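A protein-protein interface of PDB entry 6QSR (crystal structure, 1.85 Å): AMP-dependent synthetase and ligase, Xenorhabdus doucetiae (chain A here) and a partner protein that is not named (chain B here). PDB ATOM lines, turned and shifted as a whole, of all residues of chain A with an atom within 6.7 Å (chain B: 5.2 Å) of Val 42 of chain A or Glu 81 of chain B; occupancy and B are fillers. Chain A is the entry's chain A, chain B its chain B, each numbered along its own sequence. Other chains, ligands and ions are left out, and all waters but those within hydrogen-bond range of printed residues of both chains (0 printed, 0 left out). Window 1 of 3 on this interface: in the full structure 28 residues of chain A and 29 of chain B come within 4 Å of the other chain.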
ATOM      1  N   TRP A  28      28.531  -6.346 -16.095  1.00  0.00           N
ATOM      2  CA  TRP A  28      27.961  -5.171 -15.410  1.00  0.00           C
ATOM      3  C   TRP A  28      27.647  -3.984 -16.325  1.00  0.00           C
ATOM      4  O   TRP A  28      26.709  -3.233 -16.063  1.00  0.00           O
ATOM      5  CB  TRP A  28      28.925  -4.660 -14.330  1.00  0.00           C
ATOM      6  CG  TRP A  28      29.142  -5.583 -13.183  1.00  0.00           C
ATOM      7  CD1 TRP A  28      30.255  -6.325 -12.924  1.00  0.00           C
ATOM      8  CD2 TRP A  28      28.221  -5.854 -12.124  1.00  0.00           C
ATOM      9  NE1 TRP A  28      30.088  -7.042 -11.761  1.00  0.00           N
ATOM     10  CE2 TRP A  28      28.848  -6.768 -11.249  1.00  0.00           C
ATOM     11  CE3 TRP A  28      26.929  -5.406 -11.825  1.00  0.00           C
ATOM     12  CZ2 TRP A  28      28.218  -7.254 -10.094  1.00  0.00           C
ATOM     13  CZ3 TRP A  28      26.302  -5.886 -10.673  1.00  0.00           C
ATOM     14  CH2 TRP A  28      26.950  -6.800  -9.826  1.00  0.00           C
ATOM     15  N   HIS A  32      23.967  -0.860 -19.273  1.00  0.00           N
ATOM     16  CA  HIS A  32      24.225   0.075 -18.183  1.00  0.00           C
ATOM     17  C   HIS A  32      25.442   0.932 -18.560  1.00  0.00           C
ATOM     18  O   HIS A  32      26.518   0.736 -18.007  1.00  0.00           O
ATOM     19  CB  HIS A  32      24.463  -0.713 -16.885  1.00  0.00           C
ATOM     20  CG  HIS A  32      24.440   0.126 -15.645  1.00  0.00           C
ATOM     21  ND1 HIS A  32      25.489   0.937 -15.274  1.00  0.00           N
ATOM     22  CD2 HIS A  32      23.509   0.252 -14.671  1.00  0.00           C
ATOM     23  CE1 HIS A  32      25.197   1.543 -14.139  1.00  0.00           C
ATOM     24  NE2 HIS A  32      24.003   1.138 -13.747  1.00  0.00           N
ATOM     25  N   LEU A  39      30.178   1.750 -14.506  1.00  0.00           N
ATOM     26  CA  LEU A  39      30.199   0.669 -13.526  1.00  0.00           C
ATOM     27  C   LEU A  39      29.170   0.981 -12.430  1.00  0.00           C
ATOM     28  O   LEU A  39      29.276   2.029 -11.782  1.00  0.00           O
ATOM     29  CB  LEU A  39      31.602   0.531 -12.928  1.00  0.00           C
ATOM     30  CG  LEU A  39      31.857  -0.682 -12.027  1.00  0.00           C
ATOM     31  CD1 LEU A  39      31.828  -1.975 -12.824  1.00  0.00           C
ATOM     32  CD2 LEU A  39      33.182  -0.538 -11.300  1.00  0.00           C
ATOM     33  N   PRO A  40      28.158   0.095 -12.232  1.00  0.00           N
ATOM     34  CA  PRO A  40      27.196   0.322 -11.152  1.00  0.00           C
ATOM     35  C   PRO A  40      27.846   0.382  -9.765  1.00  0.00           C
ATOM     36  O   PRO A  40      28.837  -0.323  -9.511  1.00  0.00           O
ATOM     37  CB  PRO A  40      26.265  -0.901 -11.232  1.00  0.00           C
ATOM     38  CG  PRO A  40      26.423  -1.430 -12.613  1.00  0.00           C
ATOM     39  CD  PRO A  40      27.840  -1.136 -12.985  1.00  0.00           C
ATOM     40  N   GLY A  41      27.274   1.210  -8.893  1.00  0.00           N
ATOM     41  CA  GLY A  41      27.690   1.321  -7.485  1.00  0.00           C
ATOM     42  C   GLY A  41      27.655  -0.011  -6.751  1.00  0.00           C
ATOM     43  O   GLY A  41      28.550  -0.318  -5.957  1.00  0.00           O
ATOM     44  N   VAL A  42      26.625  -0.807  -7.027  1.00  0.00           N
ATOM     45  CA  VAL A  42      26.499  -2.146  -6.444  1.00  0.00           C
ATOM     46  C   VAL A  42      27.631  -3.120  -6.813  1.00  0.00           C
ATOM     47  O   VAL A  42      27.971  -3.985  -6.015  1.00  0.00           O
ATOM     48  CB  VAL A  42      25.121  -2.768  -6.763  1.00  0.00           C
ATOM     49  CG1 VAL A  42      25.014  -3.213  -8.223  1.00  0.00           C
ATOM     50  CG2 VAL A  42      24.809  -3.924  -5.822  1.00  0.00           C
ATOM     51  N   ALA A  43      28.199  -2.987  -8.012  1.00  0.00           N
ATOM     52  CA  ALA A  43      29.312  -3.840  -8.433  1.00  0.00           C
ATOM     53  C   ALA A  43      30.557  -3.576  -7.596  1.00  0.00           C
ATOM     54  O   ALA A  43      31.287  -4.509  -7.249  1.00  0.00           O
ATOM     55  CB  ALA A  43      29.612  -3.648  -9.911  1.00  0.00           C
ATOM     56  N   GLN A  44      30.765  -2.303  -7.258  1.00  0.00           N
ATOM     57  CA  GLN A  44      31.870  -1.880  -6.395  1.00  0.00           C
ATOM     58  C   GLN A  44      31.719  -2.455  -4.981  1.00  0.00           C
ATOM     59  O   GLN A  44      32.705  -2.878  -4.370  1.00  0.00           O
ATOM     60  CB  GLN A  44      31.967  -0.347  -6.358  1.00  0.00           C
ATOM     61  CG  GLN A  44      32.281   0.287  -7.717  1.00  0.00           C
ATOM     62  CD  GLN A  44      32.204   1.805  -7.686  1.00  0.00           C
ATOM     63  OE1 GLN A  44      32.847   2.451  -6.862  1.00  0.00           O
ATOM     64  NE2 GLN A  44      31.414   2.383  -8.590  1.00  0.00           N
ATOM     65  N   ILE A  45      30.487  -2.515  -4.495  1.00  0.00           N
ATOM     66  CA  ILE A  45      30.188  -3.148  -3.198  1.00  0.00           C
ATOM     67  C   ILE A  45      30.373  -4.671  -3.302  1.00  0.00           C
ATOM     68  O   ILE A  45      30.950  -5.296  -2.392  1.00  0.00           O
ATOM     69  CB  ILE A  45      28.784  -2.766  -2.695  1.00  0.00           C
ATOM     70  CG1 ILE A  45      28.734  -1.260  -2.405  1.00  0.00           C
ATOM     71  CG2 ILE A  45      28.422  -3.526  -1.420  1.00  0.00           C
ATOM     72  CD1 ILE A  45      27.354  -0.670  -2.475  1.00  0.00           C
ATOM     73  N   ASP A  46      29.914  -5.242  -4.419  1.00  0.00           N
ATOM     74  CA  ASP A  46      30.001  -6.685  -4.674  1.00  0.00           C
ATOM     75  C   ASP A  46      31.446  -7.199  -4.549  1.00  0.00           C
ATOM     76  O   ASP A  46      31.687  -8.185  -3.867  1.00  0.00           O
ATOM     77  CB  ASP A  46      29.387  -7.029  -6.043  1.00  0.00           C
ATOM     78  CG  ASP A  46      29.136  -8.519  -6.225  1.00  0.00           C
ATOM     79  OD1 ASP A  46      28.251  -9.074  -5.543  1.00  0.00           O
ATOM     80  OD2 ASP A  46      29.805  -9.138  -7.069  1.00  0.00           O
ATOM     81  N   TRP A  47      32.407  -6.496  -5.158  1.00  0.00           N
ATOM     82  CA  TRP A  47      33.812  -6.912  -5.122  1.00  0.00           C
ATOM     83  C   TRP A  47      34.453  -6.710  -3.744  1.00  0.00           C
ATOM     84  O   TRP A  47      35.214  -7.555  -3.287  1.00  0.00           O
ATOM     85  CB  TRP A  47      34.629  -6.186  -6.200  1.00  0.00           C
ATOM     86  CG  TRP A  47      34.066  -6.337  -7.581  1.00  0.00           C
ATOM     87  CD1 TRP A  47      33.294  -7.365  -8.055  1.00  0.00           C
ATOM     88  CD2 TRP A  47      34.244  -5.433  -8.676  1.00  0.00           C
ATOM     89  NE1 TRP A  47      32.960  -7.140  -9.374  1.00  0.00           N
ATOM     90  CE2 TRP A  47      33.539  -5.966  -9.781  1.00  0.00           C
ATOM     91  CE3 TRP A  47      34.925  -4.217  -8.829  1.00  0.00           C
ATOM     92  CZ2 TRP A  47      33.499  -5.323 -11.029  1.00  0.00           C
ATOM     93  CZ3 TRP A  47      34.877  -3.574 -10.074  1.00  0.00           C
ATOM     94  CH2 TRP A  47      34.166  -4.130 -11.150  1.00  0.00           C
ATOM     95  N   PHE A  70      29.763   7.523  -3.855  1.00  0.00           N
ATOM     96  CA  PHE A  70      30.289   7.327  -5.193  1.00  0.00           C
ATOM     97  C   PHE A  70      30.505   8.718  -5.751  1.00  0.00           C
ATOM     98  O   PHE A  70      29.544   9.416  -6.092  1.00  0.00           O
ATOM     99  CB  PHE A  70      29.296   6.539  -6.039  1.00  0.00           C
ATOM    100  CG  PHE A  70      28.954   5.195  -5.470  1.00  0.00           C
ATOM    101  CD1 PHE A  70      27.741   4.980  -4.815  1.00  0.00           C
ATOM    102  CD2 PHE A  70      29.858   4.146  -5.568  1.00  0.00           C
ATOM    103  CE1 PHE A  70      27.433   3.734  -4.298  1.00  0.00           C
ATOM    104  CE2 PHE A  70      29.560   2.900  -5.046  1.00  0.00           C
ATOM    105  CZ  PHE A  70      28.340   2.693  -4.409  1.00  0.00           C
ATOM    106  N   HIS B  34      18.361   1.933 -18.034  1.00  0.00           N
ATOM    107  CA  HIS B  34      18.853   0.555 -17.925  1.00  0.00           C
ATOM    108  C   HIS B  34      18.195  -0.350 -18.947  1.00  0.00           C
ATOM    109  O   HIS B  34      17.030  -0.143 -19.302  1.00  0.00           O
ATOM    110  CB  HIS B  34      18.543  -0.048 -16.537  1.00  0.00           C
ATOM    111  CG  HIS B  34      19.045   0.761 -15.379  1.00  0.00           C
ATOM    112  ND1 HIS B  34      18.581   2.030 -15.101  1.00  0.00           N
ATOM    113  CD2 HIS B  34      19.927   0.460 -14.398  1.00  0.00           C
ATOM    114  CE1 HIS B  34      19.174   2.484 -14.011  1.00  0.00           C
ATOM    115  NE2 HIS B  34      20.001   1.554 -13.572  1.00  0.00           N
ATOM    116  N   MET B  38      20.760  -5.610 -16.915  1.00  0.00           N
ATOM    117  CA  MET B  38      20.904  -4.720 -15.748  1.00  0.00           C
ATOM    118  C   MET B  38      19.613  -4.031 -15.277  1.00  0.00           C
ATOM    119  O   MET B  38      19.670  -2.966 -14.660  1.00  0.00           O
ATOM    120  CB  MET B  38      22.008  -3.679 -16.017  1.00  0.00           C
ATOM    121  CG  MET B  38      23.402  -4.247 -15.854  1.00  0.00           C
ATOM    122  SD  MET B  38      23.718  -4.884 -14.195  1.00  0.00           S
ATOM    123  CE  MET B  38      23.397  -3.440 -13.183  1.00  0.00           C
ATOM    124  N   LEU B  40      16.898  -4.850 -12.606  1.00  0.00           N
ATOM    125  CA  LEU B  40      16.769  -5.763 -11.481  1.00  0.00           C
ATOM    126  C   LEU B  40      15.391  -5.662 -10.803  1.00  0.00           C
ATOM    127  O   LEU B  40      15.249  -6.023  -9.646  1.00  0.00           O
ATOM    128  CB  LEU B  40      17.908  -5.517 -10.475  1.00  0.00           C
ATOM    129  CG  LEU B  40      19.237  -6.197 -10.826  1.00  0.00           C
ATOM    130  CD1 LEU B  40      20.012  -5.423 -11.888  1.00  0.00           C
ATOM    131  CD2 LEU B  40      20.090  -6.390  -9.584  1.00  0.00           C
ATOM    132  N   TRP B  77      23.387  -6.942  -0.165  1.00  0.00           N
ATOM    133  CA  TRP B  77      23.878  -5.673  -0.709  1.00  0.00           C
ATOM    134  C   TRP B  77      23.240  -5.229  -2.028  1.00  0.00           C
ATOM    135  O   TRP B  77      23.222  -4.026  -2.330  1.00  0.00           O
ATOM    136  CB  TRP B  77      25.411  -5.658  -0.811  1.00  0.00           C
ATOM    137  CG  TRP B  77      26.049  -6.734  -1.644  1.00  0.00           C
ATOM    138  CD1 TRP B  77      26.278  -6.706  -2.986  1.00  0.00           C
ATOM    139  CD2 TRP B  77      26.611  -7.964  -1.166  1.00  0.00           C
ATOM    140  NE1 TRP B  77      26.913  -7.851  -3.376  1.00  0.00           N
ATOM    141  CE2 TRP B  77      27.137  -8.640  -2.279  1.00  0.00           C
ATOM    142  CE3 TRP B  77      26.694  -8.571   0.099  1.00  0.00           C
ATOM    143  CZ2 TRP B  77      27.756  -9.898  -2.180  1.00  0.00           C
ATOM    144  CZ3 TRP B  77      27.317  -9.825   0.202  1.00  0.00           C
ATOM    145  CH2 TRP B  77      27.840 -10.470  -0.933  1.00  0.00           C
ATOM    146  N   PHE B  78      22.660  -6.167  -2.779  1.00  0.00           N
ATOM    147  CA  PHE B  78      21.848  -5.811  -3.958  1.00  0.00           C
ATOM    148  C   PHE B  78      20.575  -4.997  -3.640  1.00  0.00           C
ATOM    149  O   PHE B  78      19.960  -4.444  -4.549  1.00  0.00           O
ATOM    150  CB  PHE B  78      21.508  -7.055  -4.795  1.00  0.00           C
ATOM    151  CG  PHE B  78      22.667  -7.568  -5.577  1.00  0.00           C
ATOM    152  CD1 PHE B  78      22.928  -7.081  -6.847  1.00  0.00           C
ATOM    153  CD2 PHE B  78      23.547  -8.494  -5.025  1.00  0.00           C
ATOM    154  CE1 PHE B  78      24.028  -7.523  -7.558  1.00  0.00           C
ATOM    155  CE2 PHE B  78      24.649  -8.944  -5.732  1.00  0.00           C
ATOM    156  CZ  PHE B  78      24.891  -8.460  -7.008  1.00  0.00           C
ATOM    157  N   ALA B  79      20.175  -4.935  -2.367  1.00  0.00           N
ATOM    158  CA  ALA B  79      19.139  -4.014  -1.911  1.00  0.00           C
ATOM    159  C   ALA B  79      19.337  -2.569  -2.389  1.00  0.00           C
ATOM    160  O   ALA B  79      18.369  -1.907  -2.774  1.00  0.00           O
ATOM    161  CB  ALA B  79      19.035  -4.051  -0.385  1.00  0.00           C
ATOM    162  N   ILE B  80      20.575  -2.078  -2.375  1.00  0.00           N
ATOM    163  CA  ILE B  80      20.826  -0.710  -2.827  1.00  0.00           C
ATOM    164  C   ILE B  80      20.515  -0.511  -4.310  1.00  0.00           C
ATOM    165  O   ILE B  80      19.988   0.543  -4.687  1.00  0.00           O
ATOM    166  CB  ILE B  80      22.249  -0.186  -2.511  1.00  0.00           C
ATOM    167  CG1 ILE B  80      23.351  -1.032  -3.156  1.00  0.00           C
ATOM    168  CG2 ILE B  80      22.437  -0.121  -1.011  1.00  0.00           C
ATOM    169  CD1 ILE B  80      24.286  -0.254  -4.053  1.00  0.00           C
ATOM    170  N   GLU B  81      20.801  -1.523  -5.132  1.00  0.00           N
ATOM    171  CA  GLU B  81      20.532  -1.457  -6.571  1.00  0.00           C
ATOM    172  C   GLU B  81      19.043  -1.599  -6.883  1.00  0.00           C
ATOM    173  O   GLU B  81      18.544  -0.944  -7.790  1.00  0.00           O
ATOM    174  CB  GLU B  81      21.324  -2.522  -7.341  1.00  0.00           C
ATOM    175  CG  GLU B  81      21.197  -2.456  -8.870  1.00  0.00           C
ATOM    176  CD  GLU B  81      21.714  -1.160  -9.488  1.00  0.00           C
ATOM    177  OE1 GLU B  81      22.470  -0.426  -8.821  1.00  0.00           O
ATOM    178  OE2 GLU B  81      21.371  -0.868 -10.655  1.00  0.00           O
ATOM    179  N   MET B  82      18.342  -2.468  -6.162  1.00  0.00           N
ATOM    180  CA  MET B  82      16.896  -2.568  -6.316  1.00  0.00           C
ATOM    181  C   MET B  82      16.215  -1.249  -5.875  1.00  0.00           C
ATOM    182  O   MET B  82      15.340  -0.737  -6.567  1.00  0.00           O
ATOM    183  CB  MET B  82      16.348  -3.786  -5.566  1.00  0.00           C
ATOM    184  CG  MET B  82      16.798  -5.134  -6.151  1.00  0.00           C
ATOM    185  SD  MET B  82      16.083  -6.550  -5.285  1.00  0.00           S
ATOM    186  CE  MET B  82      17.076  -6.515  -3.801  1.00  0.00           C
ATOM    187  N   MET B  83      16.658  -0.678  -4.755  1.00  0.00           N
ATOM    188  CA  MET B  83      16.143   0.625  -4.289  1.00  0.00           C
ATOM    189  C   MET B  83      16.469   1.772  -5.244  1.00  0.00           C
ATOM    190  O   MET B  83      15.612   2.632  -5.510  1.00  0.00           O
ATOM    191  CB  MET B  83      16.654   0.929  -2.882  1.00  0.00           C
ATOM    192  CG  MET B  83      15.959   0.108  -1.813  1.00  0.00           C
ATOM    193  SD  MET B  83      16.560   0.488  -0.152  1.00  0.00           S
ATOM    194  CE  MET B  83      17.904  -0.664  -0.012  1.00  0.00           C
ATOM    195  N   ALA B  84      17.690   1.766  -5.773  1.00  0.00           N
ATOM    196  CA  ALA B  84      18.124   2.764  -6.747  1.00  0.00           C
ATOM    197  C   ALA B  84      17.263   2.723  -8.000  1.00  0.00           C
ATOM    198  O   ALA B  84      16.814   3.773  -8.494  1.00  0.00           O
ATOM    199  CB  ALA B  84      19.585   2.553  -7.112  1.00  0.00           C
ATOM    200  N   GLN B  85      17.009   1.517  -8.497  1.00  0.00           N
ATOM    201  CA  GLN B  85      16.188   1.358  -9.694  1.00  0.00           C
ATOM    202  C   GLN B  85      14.732   1.731  -9.465  1.00  0.00           C
ATOM    203  O   GLN B  85      14.106   2.263 -10.368  1.00  0.00           O
ATOM    204  CB  GLN B  85      16.327  -0.044 -10.287  1.00  0.00           C
ATOM    205  CG  GLN B  85      17.663  -0.213 -10.984  1.00  0.00           C
ATOM    206  CD  GLN B  85      17.809  -1.522 -11.728  1.00  0.00           C
ATOM    207  OE1 GLN B  85      16.823  -2.146 -12.127  1.00  0.00           O
ATOM    208  NE2 GLN B  85      19.049  -1.942 -11.926  1.00  0.00           N
ATOM    209  N   ALA B  86      14.209   1.496  -8.260  1.00  0.00           N
ATOM    210  CA  ALA B  86      12.867   1.958  -7.915  1.00  0.00           C
ATOM    211  C   ALA B  86      12.761   3.481  -8.008  1.00  0.00           C
ATOM    212  O   ALA B  86      11.765   3.999  -8.506  1.00  0.00           O
ATOM    213  CB  ALA B  86      12.463   1.482  -6.522  1.00  0.00           C
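The side-chain carboxylate (OD1) of Asp 46 of chain A sits at hydrogen-bond distance from the indole nitrogen (NE1) of Trp 77 of chain B, 2.8 Å away.
The side-chain carboxylate of Glu 81 of chain B sits at hydrogen-bond distance from the side-chain amide nitrogen of Gln 85 of chain B, at 2.9 Å. The backbone carbonyl oxygen (O) of Met 38 of chain B sits at hydrogen-bond distance from the side-chain amide nitrogen (NE2) of Gln 85 of chain B, 3.0 Å away.
Among the printed residues, merely in contact across the chains: Trp 28 of chain A with Met 38 of chain B (3.5 Å), Trp 28 of chain A with Phe 78 of chain B (3.8 Å), His 32 of chain A with His 34 of chain B (3.6 Å), His 32 of chain A with Met 38 of chain B (3.8 Å), Pro 40 of chain A with Met 38 of chain B (3.7 Å), Val 42 of chain A with Trp 77 of chain B (3.8 Å), Val 42 of chain A with Phe 78 of chain B (3.8 Å), Val 42 of chain A with Ile 80 of chain B (3.8 Å), Val 42 of chain A with Glu 81 of chain B (3.8 Å), Ile 45 of chain A with Trp 77 of chain B (3.7 Å), Ile 45 of chain A with Ile 80 of chain B (3.5 Å) and Asp 46 of chain A with Phe 78 of chain B (3.6 Å).
Of the printed residues of chain B, His 32 of chain A touches His 34 and Met 38. Of the printed residues of chain B, Pro 40 of chain A touches Met 38. Val 42 of chain A touches just these residues of chain B: Trp 77, Phe 78, Ile 80 and Glu 81. Of the printed residues of chain B, Asp 46 of chain A touches Trp 77 and Phe 78. Phe 70 of chain A touches none of the printed residues of chain B. Of the printed residues of chain A, Phe 78 of chain B touches Trp 28, Val 42 and Asp 46. Of the printed residues of chain A, Ile 80 of chain B touches Val 42 (3.8 Å) and Ile 45 (3.5 Å). Of the printed residues of chain A, Glu 81 of chain B touches Val 42. The nearest printed residue of chain B that does not touch Val 42 of chain A is Met 38 of chain B (5.2 Å). The nearest printed residue of chain A that does not touch Glu 81 of chain B is Pro 40 of chain A (4.5 Å). The nearest printed residue of chain A that does not touch Phe 78 of chain B is Ala 43 of chain A (6.2 Å).
Of the 13 printed residues of chain B, 6 touch a printed residue of chain A. Hydrophobic or aromatic side chains of chain B that line the printed part of chain A: His 34, Met 38, Trp 77, Phe 78 and Ile 80. Among the printed residues, 13 pairs touch across the chains.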
